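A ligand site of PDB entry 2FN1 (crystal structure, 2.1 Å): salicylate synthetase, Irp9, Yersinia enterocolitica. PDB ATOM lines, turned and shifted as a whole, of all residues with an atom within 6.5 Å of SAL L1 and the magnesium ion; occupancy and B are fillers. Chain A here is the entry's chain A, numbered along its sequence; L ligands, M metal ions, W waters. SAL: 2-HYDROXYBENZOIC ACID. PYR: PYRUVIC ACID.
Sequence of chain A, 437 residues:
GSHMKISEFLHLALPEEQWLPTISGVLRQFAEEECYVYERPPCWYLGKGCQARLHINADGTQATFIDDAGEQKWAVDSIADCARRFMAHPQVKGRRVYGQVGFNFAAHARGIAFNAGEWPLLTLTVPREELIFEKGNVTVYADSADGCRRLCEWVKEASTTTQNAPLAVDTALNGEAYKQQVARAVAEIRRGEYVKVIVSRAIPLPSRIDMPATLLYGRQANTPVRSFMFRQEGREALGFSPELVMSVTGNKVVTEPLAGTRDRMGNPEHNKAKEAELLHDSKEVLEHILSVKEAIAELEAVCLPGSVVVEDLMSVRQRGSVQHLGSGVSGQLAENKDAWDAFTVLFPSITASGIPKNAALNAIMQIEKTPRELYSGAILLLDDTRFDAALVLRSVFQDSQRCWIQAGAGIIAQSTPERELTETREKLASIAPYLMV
Within 4 Å of the magnesium ion: Glu 287 and Glu 423. Along chain A the residues within 4 Å of the magnesium ion span positions 287 to 423. The nearest printed residue that does not touch the magnesium ion is Gly 260 (4.01 Å).
O of Gly 408 lies within hydrogen-bond range of NZ of Lys 427 (2.9 Å). The backbone NH of Ala 259 sits at hydrogen-bond distance from the backbone carbonyl oxygen of Leu 325 (3.0 Å). O of Leu 258 sits close to OG1 of Thr 351 (3.4 Å). NZ of Lys 427 sits close to OE2 of Glu 423, 3.1 Å away. The side-chain hydroxyl of Thr 261 sits at hydrogen-bond distance from a ring nitrogen (ND1) of His 324. O of Gly 260 lies within hydrogen-bond range of N of Leu 325, at 3.2 Å. The side-chain hydroxyl (OG1) of Thr 351 is in hydrogen-bond range of the side-chain carboxylate (OE2) of Glu 243 (2.7 Å). NH1 of Arg 394 is in hydrogen-bond range of NE2 of His 324.
Ile 198 touches SAL L1 (CG1 to O2, 3.8 Å). Glu 243 touches SAL L1. Leu 258 touches SAL L1. Ala 259 touches SAL L1 (C to O2', 3.6 Å). His 324 touches SAL L1. CD1 of Leu 393 touches C4 of SAL L1, at 3.8 Å. Arg 394 touches SAL L1 (NH2 to C5, 3.4 Å). Hydrophobic or aromatic side chains within 4 Å of SAL L1: Ile 198, His 324 and Leu 393.
O of Thr 351 sits at hydrogen-bond distance from O2 of SAL L1, 3.0 Å away. N of Gly 410 lies close to O1' of SAL L1, at 3.1 Å. The side-chain hydroxyl (OG1) of Thr 261 sits close to an oxygen (O2') of SAL L1 (2.8 Å). The side-chain amino group (NZ) of Lys 427 lies close to an oxygen (O1') of SAL L1 (3.1 Å). An oxygen (O2') of SAL L1 lies close to the backbone NH (N) of Gly 260 (2.6 Å). The guanidinium group (NE) of Arg 394 is in salt-bridge range of an oxygen (OXT) of PYR L2 (2.6 Å). An oxygen (O) of PYR L2 is in hydrogen-bond range of the backbone NH (N) of Gly 408. NZ of Lys 427 is in hydrogen-bond range of O3 of PYR L2.
The magnesium ion is bound by water W1, water W3, OE2 of Glu 287, O2' of SAL L1, O1' of SAL L1 and OE2 of Glu 423. The magnesium ion has six donor atoms within binding distance.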
ATOM      1  N   LYS A 196     -25.141 -17.770 -21.219  1.00  0.00           N
ATOM      2  CA  LYS A 196     -24.477 -17.366 -19.980  1.00  0.00           C
ATOM      3  C   LYS A 196     -25.504 -17.095 -18.910  1.00  0.00           C
ATOM      4  O   LYS A 196     -26.532 -16.485 -19.181  1.00  0.00           O
ATOM      5  CB  LYS A 196     -23.595 -16.110 -20.205  1.00  0.00           C
ATOM      6  CG  LYS A 196     -22.981 -15.538 -18.907  1.00  0.00           C
ATOM      7  CD  LYS A 196     -22.415 -14.110 -19.008  1.00  0.00           C
ATOM      8  CE  LYS A 196     -20.944 -14.038 -19.400  1.00  0.00           C
ATOM      9  NZ  LYS A 196     -20.272 -12.847 -18.715  1.00  0.00           N
ATOM     10  N   ILE A 198     -25.476 -15.845 -14.563  1.00  0.00           N
ATOM     11  CA  ILE A 198     -24.839 -15.620 -13.286  1.00  0.00           C
ATOM     12  C   ILE A 198     -25.584 -16.375 -12.178  1.00  0.00           C
ATOM     13  O   ILE A 198     -26.758 -16.094 -11.895  1.00  0.00           O
ATOM     14  CB  ILE A 198     -24.662 -14.118 -12.962  1.00  0.00           C
ATOM     15  CG1 ILE A 198     -23.492 -13.468 -13.764  1.00  0.00           C
ATOM     16  CG2 ILE A 198     -24.325 -13.940 -11.474  1.00  0.00           C
ATOM     17  CD1 ILE A 198     -23.634 -13.406 -15.362  1.00  0.00           C
ATOM     18  N   PRO A 242     -18.408  -2.572  -8.111  1.00  0.00           N
ATOM     19  CA  PRO A 242     -17.279  -2.672  -9.023  1.00  0.00           C
ATOM     20  C   PRO A 242     -17.517  -2.028 -10.401  1.00  0.00           C
ATOM     21  O   PRO A 242     -16.564  -1.801 -11.136  1.00  0.00           O
ATOM     22  CB  PRO A 242     -17.059  -4.207  -9.160  1.00  0.00           C
ATOM     23  CG  PRO A 242     -18.432  -4.845  -8.868  1.00  0.00           C
ATOM     24  CD  PRO A 242     -19.239  -3.810  -8.072  1.00  0.00           C
ATOM     25  N   GLU A 243     -18.765  -1.703 -10.742  1.00  0.00           N
ATOM     26  CA  GLU A 243     -19.065  -1.192 -12.079  1.00  0.00           C
ATOM     27  C   GLU A 243     -20.386  -0.469 -12.106  1.00  0.00           C
ATOM     28  O   GLU A 243     -21.241  -0.654 -11.246  1.00  0.00           O
ATOM     29  CB  GLU A 243     -19.055  -2.303 -13.128  1.00  0.00           C
ATOM     30  CG  GLU A 243     -20.311  -3.179 -13.112  1.00  0.00           C
ATOM     31  CD  GLU A 243     -20.096  -4.550 -13.700  1.00  0.00           C
ATOM     32  OE1 GLU A 243     -19.430  -5.361 -13.013  1.00  0.00           O
ATOM     33  OE2 GLU A 243     -20.593  -4.806 -14.831  1.00  0.00           O
ATOM     34  N   LEU A 258     -18.155  -5.555 -16.674  1.00  0.00           N
ATOM     35  CA  LEU A 258     -16.973  -6.254 -16.167  1.00  0.00           C
ATOM     36  C   LEU A 258     -17.370  -7.735 -16.109  1.00  0.00           C
ATOM     37  O   LEU A 258     -18.493  -8.081 -15.706  1.00  0.00           O
ATOM     38  CB  LEU A 258     -16.524  -5.688 -14.801  1.00  0.00           C
ATOM     39  CG  LEU A 258     -15.480  -4.532 -14.782  1.00  0.00           C
ATOM     40  CD1 LEU A 258     -15.898  -3.240 -15.532  1.00  0.00           C
ATOM     41  CD2 LEU A 258     -15.105  -4.164 -13.351  1.00  0.00           C
ATOM     42  N   ALA A 259     -16.481  -8.601 -16.603  1.00  0.00           N
ATOM     43  CA  ALA A 259     -16.719 -10.037 -16.688  1.00  0.00           C
ATOM     44  C   ALA A 259     -15.357 -10.658 -16.924  1.00  0.00           C
ATOM     45  O   ALA A 259     -14.604 -10.224 -17.790  1.00  0.00           O
ATOM     46  CB  ALA A 259     -17.667 -10.389 -17.843  1.00  0.00           C
ATOM     47  N   GLY A 260     -15.038 -11.684 -16.164  1.00  0.00           N
ATOM     48  CA  GLY A 260     -13.741 -12.319 -16.297  1.00  0.00           C
ATOM     49  C   GLY A 260     -13.008 -11.890 -15.028  1.00  0.00           C
ATOM     50  O   GLY A 260     -12.906 -10.716 -14.729  1.00  0.00           O
ATOM     51  N   THR A 261     -12.505 -12.844 -14.271  1.00  0.00           N
ATOM     52  CA  THR A 261     -11.983 -12.534 -12.940  1.00  0.00           C
ATOM     53  C   THR A 261     -10.733 -13.349 -12.650  1.00  0.00           C
ATOM     54  O   THR A 261     -10.646 -14.508 -13.030  1.00  0.00           O
ATOM     55  CB  THR A 261     -13.094 -12.864 -11.875  1.00  0.00           C
ATOM     56  OG1 THR A 261     -14.180 -11.943 -12.077  1.00  0.00           O
ATOM     57  CG2 THR A 261     -12.581 -12.728 -10.425  1.00  0.00           C
ATOM     58  N   LYS A 283     -11.140 -18.714 -21.769  1.00  0.00           N
ATOM     59  CA  LYS A 283     -12.438 -18.779 -21.086  1.00  0.00           C
ATOM     60  C   LYS A 283     -12.809 -17.394 -20.565  1.00  0.00           C
ATOM     61  O   LYS A 283     -13.907 -16.929 -20.832  1.00  0.00           O
ATOM     62  CB  LYS A 283     -12.429 -19.832 -19.969  1.00  0.00           C
ATOM     63  CG  LYS A 283     -13.750 -20.031 -19.193  1.00  0.00           C
ATOM     64  CD  LYS A 283     -13.926 -19.063 -18.050  1.00  0.00           C
ATOM     65  CE  LYS A 283     -15.217 -19.342 -17.278  1.00  0.00           C
ATOM     66  NZ  LYS A 283     -15.343 -18.356 -16.186  1.00  0.00           N
ATOM     67  N   GLU A 284     -11.879 -16.731 -19.871  1.00  0.00           N
ATOM     68  CA  GLU A 284     -12.178 -15.399 -19.335  1.00  0.00           C
ATOM     69  C   GLU A 284     -12.419 -14.360 -20.431  1.00  0.00           C
ATOM     70  O   GLU A 284     -13.290 -13.494 -20.298  1.00  0.00           O
ATOM     71  CB  GLU A 284     -11.042 -14.904 -18.444  1.00  0.00           C
ATOM     72  CG  GLU A 284     -10.687 -15.883 -17.304  1.00  0.00           C
ATOM     73  CD  GLU A 284     -11.850 -16.119 -16.354  1.00  0.00           C
ATOM     74  OE1 GLU A 284     -12.661 -15.214 -16.135  1.00  0.00           O
ATOM     75  OE2 GLU A 284     -11.941 -17.220 -15.802  1.00  0.00           O
ATOM     76  N   GLU A 287     -15.938 -15.184 -22.048  1.00  0.00           N
ATOM     77  CA  GLU A 287     -16.905 -14.647 -21.078  1.00  0.00           C
ATOM     78  C   GLU A 287     -17.015 -13.135 -21.201  1.00  0.00           C
ATOM     79  O   GLU A 287     -18.118 -12.576 -21.276  1.00  0.00           O
ATOM     80  CB  GLU A 287     -16.414 -14.979 -19.674  1.00  0.00           C
ATOM     81  CG  GLU A 287     -17.436 -14.762 -18.513  1.00  0.00           C
ATOM     82  CD  GLU A 287     -16.830 -15.227 -17.196  1.00  0.00           C
ATOM     83  OE1 GLU A 287     -16.020 -16.184 -17.243  1.00  0.00           O
ATOM     84  OE2 GLU A 287     -17.127 -14.625 -16.126  1.00  0.00           O
ATOM     85  N   HIS A 324     -10.670  -7.624 -12.773  1.00  0.00           N
ATOM     86  CA  HIS A 324     -11.637  -8.122 -13.777  1.00  0.00           C
ATOM     87  C   HIS A 324     -11.271  -7.528 -15.085  1.00  0.00           C
ATOM     88  O   HIS A 324     -10.730  -6.439 -15.118  1.00  0.00           O
ATOM     89  CB  HIS A 324     -13.074  -7.632 -13.506  1.00  0.00           C
ATOM     90  CG  HIS A 324     -13.598  -7.943 -12.143  1.00  0.00           C
ATOM     91  ND1 HIS A 324     -13.861  -9.234 -11.721  1.00  0.00           N
ATOM     92  CD2 HIS A 324     -13.916  -7.127 -11.097  1.00  0.00           C
ATOM     93  CE1 HIS A 324     -14.342  -9.203 -10.481  1.00  0.00           C
ATOM     94  NE2 HIS A 324     -14.378  -7.935 -10.074  1.00  0.00           N
ATOM     95  N   LEU A 325     -11.659  -8.189 -16.170  1.00  0.00           N
ATOM     96  CA  LEU A 325     -11.685  -7.511 -17.486  1.00  0.00           C
ATOM     97  C   LEU A 325     -12.878  -6.580 -17.538  1.00  0.00           C
ATOM     98  O   LEU A 325     -13.979  -6.938 -17.118  1.00  0.00           O
ATOM     99  CB  LEU A 325     -11.734  -8.522 -18.614  1.00  0.00           C
ATOM    100  CG  LEU A 325     -10.602  -9.575 -18.604  1.00  0.00           C
ATOM    101  CD1 LEU A 325     -10.828 -10.781 -19.529  1.00  0.00           C
ATOM    102  CD2 LEU A 325      -9.257  -8.889 -18.941  1.00  0.00           C
ATOM    103  N   THR A 351     -23.733  -8.523 -16.946  1.00  0.00           N
ATOM    104  CA  THR A 351     -22.695  -9.221 -16.179  1.00  0.00           C
ATOM    105  C   THR A 351     -23.167  -9.693 -14.775  1.00  0.00           C
ATOM    106  O   THR A 351     -22.454 -10.415 -14.110  1.00  0.00           O
ATOM    107  CB  THR A 351     -21.452  -8.337 -16.077  1.00  0.00           C
ATOM    108  OG1 THR A 351     -21.780  -7.137 -15.368  1.00  0.00           O
ATOM    109  CG2 THR A 351     -20.901  -7.986 -17.487  1.00  0.00           C
ATOM    110  N   ALA A 352     -24.386  -9.301 -14.375  1.00  0.00           N
ATOM    111  CA  ALA A 352     -25.052  -9.822 -13.162  1.00  0.00           C
ATOM    112  C   ALA A 352     -26.306 -10.690 -13.421  1.00  0.00           C
ATOM    113  O   ALA A 352     -26.961 -11.163 -12.488  1.00  0.00           O
ATOM    114  CB  ALA A 352     -25.379  -8.702 -12.238  1.00  0.00           C
ATOM    115  N   LEU A 391     -23.891  -0.892 -10.017  1.00  0.00           N
ATOM    116  CA  LEU A 391     -24.309  -2.259  -9.843  1.00  0.00           C
ATOM    117  C   LEU A 391     -24.121  -2.736  -8.407  1.00  0.00           C
ATOM    118  O   LEU A 391     -23.063  -2.500  -7.784  1.00  0.00           O
ATOM    119  CB  LEU A 391     -23.539  -3.168 -10.827  1.00  0.00           C
ATOM    120  CG  LEU A 391     -23.877  -4.653 -10.761  1.00  0.00           C
ATOM    121  CD1 LEU A 391     -25.343  -4.938 -11.076  1.00  0.00           C
ATOM    122  CD2 LEU A 391     -22.951  -5.371 -11.732  1.00  0.00           C
ATOM    123  N   LEU A 393     -23.090  -5.298  -6.299  1.00  0.00           N
ATOM    124  CA  LEU A 393     -22.292  -6.468  -5.976  1.00  0.00           C
ATOM    125  C   LEU A 393     -21.292  -6.058  -4.884  1.00  0.00           C
ATOM    126  O   LEU A 393     -21.119  -4.863  -4.613  1.00  0.00           O
ATOM    127  CB  LEU A 393     -21.522  -6.984  -7.212  1.00  0.00           C
ATOM    128  CG  LEU A 393     -22.255  -7.277  -8.539  1.00  0.00           C
ATOM    129  CD1 LEU A 393     -21.255  -7.472  -9.695  1.00  0.00           C
ATOM    130  CD2 LEU A 393     -23.190  -8.454  -8.412  1.00  0.00           C
ATOM    131  N   ARG A 394     -20.606  -7.037  -4.309  1.00  0.00           N
ATOM    132  CA  ARG A 394     -19.588  -6.761  -3.247  1.00  0.00           C
ATOM    133  C   ARG A 394     -20.286  -5.973  -2.117  1.00  0.00           C
ATOM    134  O   ARG A 394     -19.797  -4.939  -1.679  1.00  0.00           O
ATOM    135  CB  ARG A 394     -18.374  -5.993  -3.817  1.00  0.00           C
ATOM    136  CG  ARG A 394     -17.912  -6.454  -5.252  1.00  0.00           C
ATOM    137  CD  ARG A 394     -17.551  -7.976  -5.300  1.00  0.00           C
ATOM    138  NE  ARG A 394     -17.778  -8.575  -6.648  1.00  0.00           N
ATOM    139  CZ  ARG A 394     -17.031  -8.335  -7.733  1.00  0.00           C
ATOM    140  NH1 ARG A 394     -15.989  -7.511  -7.692  1.00  0.00           N
ATOM    141  NH2 ARG A 394     -17.334  -8.894  -8.885  1.00  0.00           N
ATOM    142  N   GLY A 408     -21.664 -14.169  -6.947  1.00  0.00           N
ATOM    143  CA  GLY A 408     -21.877 -15.181  -7.941  1.00  0.00           C
ATOM    144  C   GLY A 408     -20.769 -15.204  -8.955  1.00  0.00           C
ATOM    145  O   GLY A 408     -19.719 -14.612  -8.731  1.00  0.00           O
ATOM    146  N   ALA A 409     -21.014 -15.897 -10.053  1.00  0.00           N
ATOM    147  CA  ALA A 409     -20.022 -16.056 -11.079  1.00  0.00           C
ATOM    148  C   ALA A 409     -20.794 -16.217 -12.367  1.00  0.00           C
ATOM    149  O   ALA A 409     -21.870 -16.837 -12.355  1.00  0.00           O
ATOM    150  CB  ALA A 409     -19.187 -17.313 -10.795  1.00  0.00           C
ATOM    151  N   GLY A 410     -20.236 -15.689 -13.462  1.00  0.00           N
ATOM    152  CA  GLY A 410     -20.799 -15.863 -14.800  1.00  0.00           C
ATOM    153  C   GLY A 410     -20.495 -17.238 -15.326  1.00  0.00           C
ATOM    154  O   GLY A 410     -19.335 -17.589 -15.516  1.00  0.00           O
ATOM    155  N   ILE A 411     -21.544 -18.045 -15.517  1.00  0.00           N
ATOM    156  CA  ILE A 411     -21.404 -19.411 -15.991  1.00  0.00           C
ATOM    157  C   ILE A 411     -21.609 -19.488 -17.511  1.00  0.00           C
ATOM    158  O   ILE A 411     -22.632 -19.029 -18.028  1.00  0.00           O
ATOM    159  CB  ILE A 411     -22.374 -20.416 -15.222  1.00  0.00           C
ATOM    160  CG1 ILE A 411     -22.412 -20.114 -13.716  1.00  0.00           C
ATOM    161  CG2 ILE A 411     -22.014 -21.863 -15.551  1.00  0.00           C
ATOM    162  CD1 ILE A 411     -21.079 -20.064 -13.015  1.00  0.00           C
ATOM    163  N   GLU A 420     -15.636 -21.829 -10.351  1.00  0.00           N
ATOM    164  CA  GLU A 420     -16.698 -20.857 -10.042  1.00  0.00           C
ATOM    165  C   GLU A 420     -16.985 -20.717  -8.525  1.00  0.00           C
ATOM    166  O   GLU A 420     -17.167 -19.600  -8.055  1.00  0.00           O
ATOM    167  CB  GLU A 420     -17.962 -21.178 -10.841  1.00  0.00           C
ATOM    168  CG  GLU A 420     -17.721 -21.385 -12.365  1.00  0.00           C
ATOM    169  CD  GLU A 420     -17.244 -20.130 -13.128  1.00  0.00           C
ATOM    170  OE1 GLU A 420     -17.014 -19.051 -12.523  1.00  0.00           O
ATOM    171  OE2 GLU A 420     -17.092 -20.226 -14.355  1.00  0.00           O
ATOM    172  N   GLU A 423     -14.179 -18.649  -7.393  1.00  0.00           N
ATOM    173  CA  GLU A 423     -14.428 -17.281  -7.856  1.00  0.00           C
ATOM    174  C   GLU A 423     -15.341 -16.468  -6.917  1.00  0.00           C
ATOM    175  O   GLU A 423     -15.049 -15.304  -6.626  1.00  0.00           O
ATOM    176  CB  GLU A 423     -14.934 -17.260  -9.306  1.00  0.00           C
ATOM    177  CG  GLU A 423     -14.923 -15.853  -9.845  1.00  0.00           C
ATOM    178  CD  GLU A 423     -15.049 -15.764 -11.367  1.00  0.00           C
ATOM    179  OE1 GLU A 423     -14.129 -16.213 -12.088  1.00  0.00           O
ATOM    180  OE2 GLU A 423     -16.046 -15.191 -11.835  1.00  0.00           O
ATOM    181  N   LYS A 427     -14.397 -13.087  -4.727  1.00  0.00           N
ATOM    182  CA  LYS A 427     -15.282 -11.911  -4.704  1.00  0.00           C
ATOM    183  C   LYS A 427     -15.813 -11.565  -3.274  1.00  0.00           C
ATOM    184  O   LYS A 427     -15.879 -10.381  -2.899  1.00  0.00           O
ATOM    185  CB  LYS A 427     -16.463 -12.151  -5.676  1.00  0.00           C
ATOM    186  CG  LYS A 427     -16.050 -12.090  -7.182  1.00  0.00           C
ATOM    187  CD  LYS A 427     -17.108 -12.699  -8.091  1.00  0.00           C
ATOM    188  CE  LYS A 427     -16.708 -12.585  -9.537  1.00  0.00           C
ATOM    189  NZ  LYS A 427     -17.801 -13.129 -10.401  1.00  0.00           N
HETATM  190  C1' SAL L   1     -17.238 -12.510 -13.524  1.00  0.00           C
HETATM  191  O1' SAL L   1     -18.016 -13.522 -13.446  1.00  0.00           O
HETATM  192  O2' SAL L   1     -16.081 -12.655 -13.983  1.00  0.00           O
HETATM  193  C1  SAL L   1     -17.698 -11.160 -13.077  1.00  0.00           C
HETATM  194  C2  SAL L   1     -19.171 -10.897 -12.966  1.00  0.00           C
HETATM  195  C3  SAL L   1     -19.641  -9.646 -12.545  1.00  0.00           C
HETATM  196  C4  SAL L   1     -18.714  -8.636 -12.215  1.00  0.00           C
HETATM  197  C5  SAL L   1     -17.339  -8.896 -12.314  1.00  0.00           C
HETATM  198  C6  SAL L   1     -16.834 -10.133 -12.756  1.00  0.00           C
HETATM  199  O2  SAL L   1     -20.012 -11.906 -13.280  1.00  0.00           O
HETATM  200  C   PYR L   2     -20.622 -10.900  -7.932  1.00  0.00           C
HETATM  201  O   PYR L   2     -21.634 -11.333  -7.216  1.00  0.00           O
HETATM  202  OXT PYR L   2     -19.726 -10.152  -7.358  1.00  0.00           O
HETATM  203  CA  PYR L   2     -20.450 -11.204  -9.284  1.00  0.00           C
HETATM  204  O3  PYR L   2     -19.311 -10.938  -9.833  1.00  0.00           O
HETATM  205  CB  PYR L   2     -21.525 -11.793 -10.134  1.00  0.00           C
HETATM  206 MG    MG M   1     -16.344 -14.851 -14.082  1.00  0.00          MG
HETATM  207  O   HOH W   1     -14.487 -15.305 -14.332  1.00  0.00           O
HETATM  208  O   HOH W   2     -19.394 -13.314 -16.491  1.00  0.00           O
HETATM  209  O   HOH W   3     -17.156 -16.690 -14.154  1.00  0.00           O
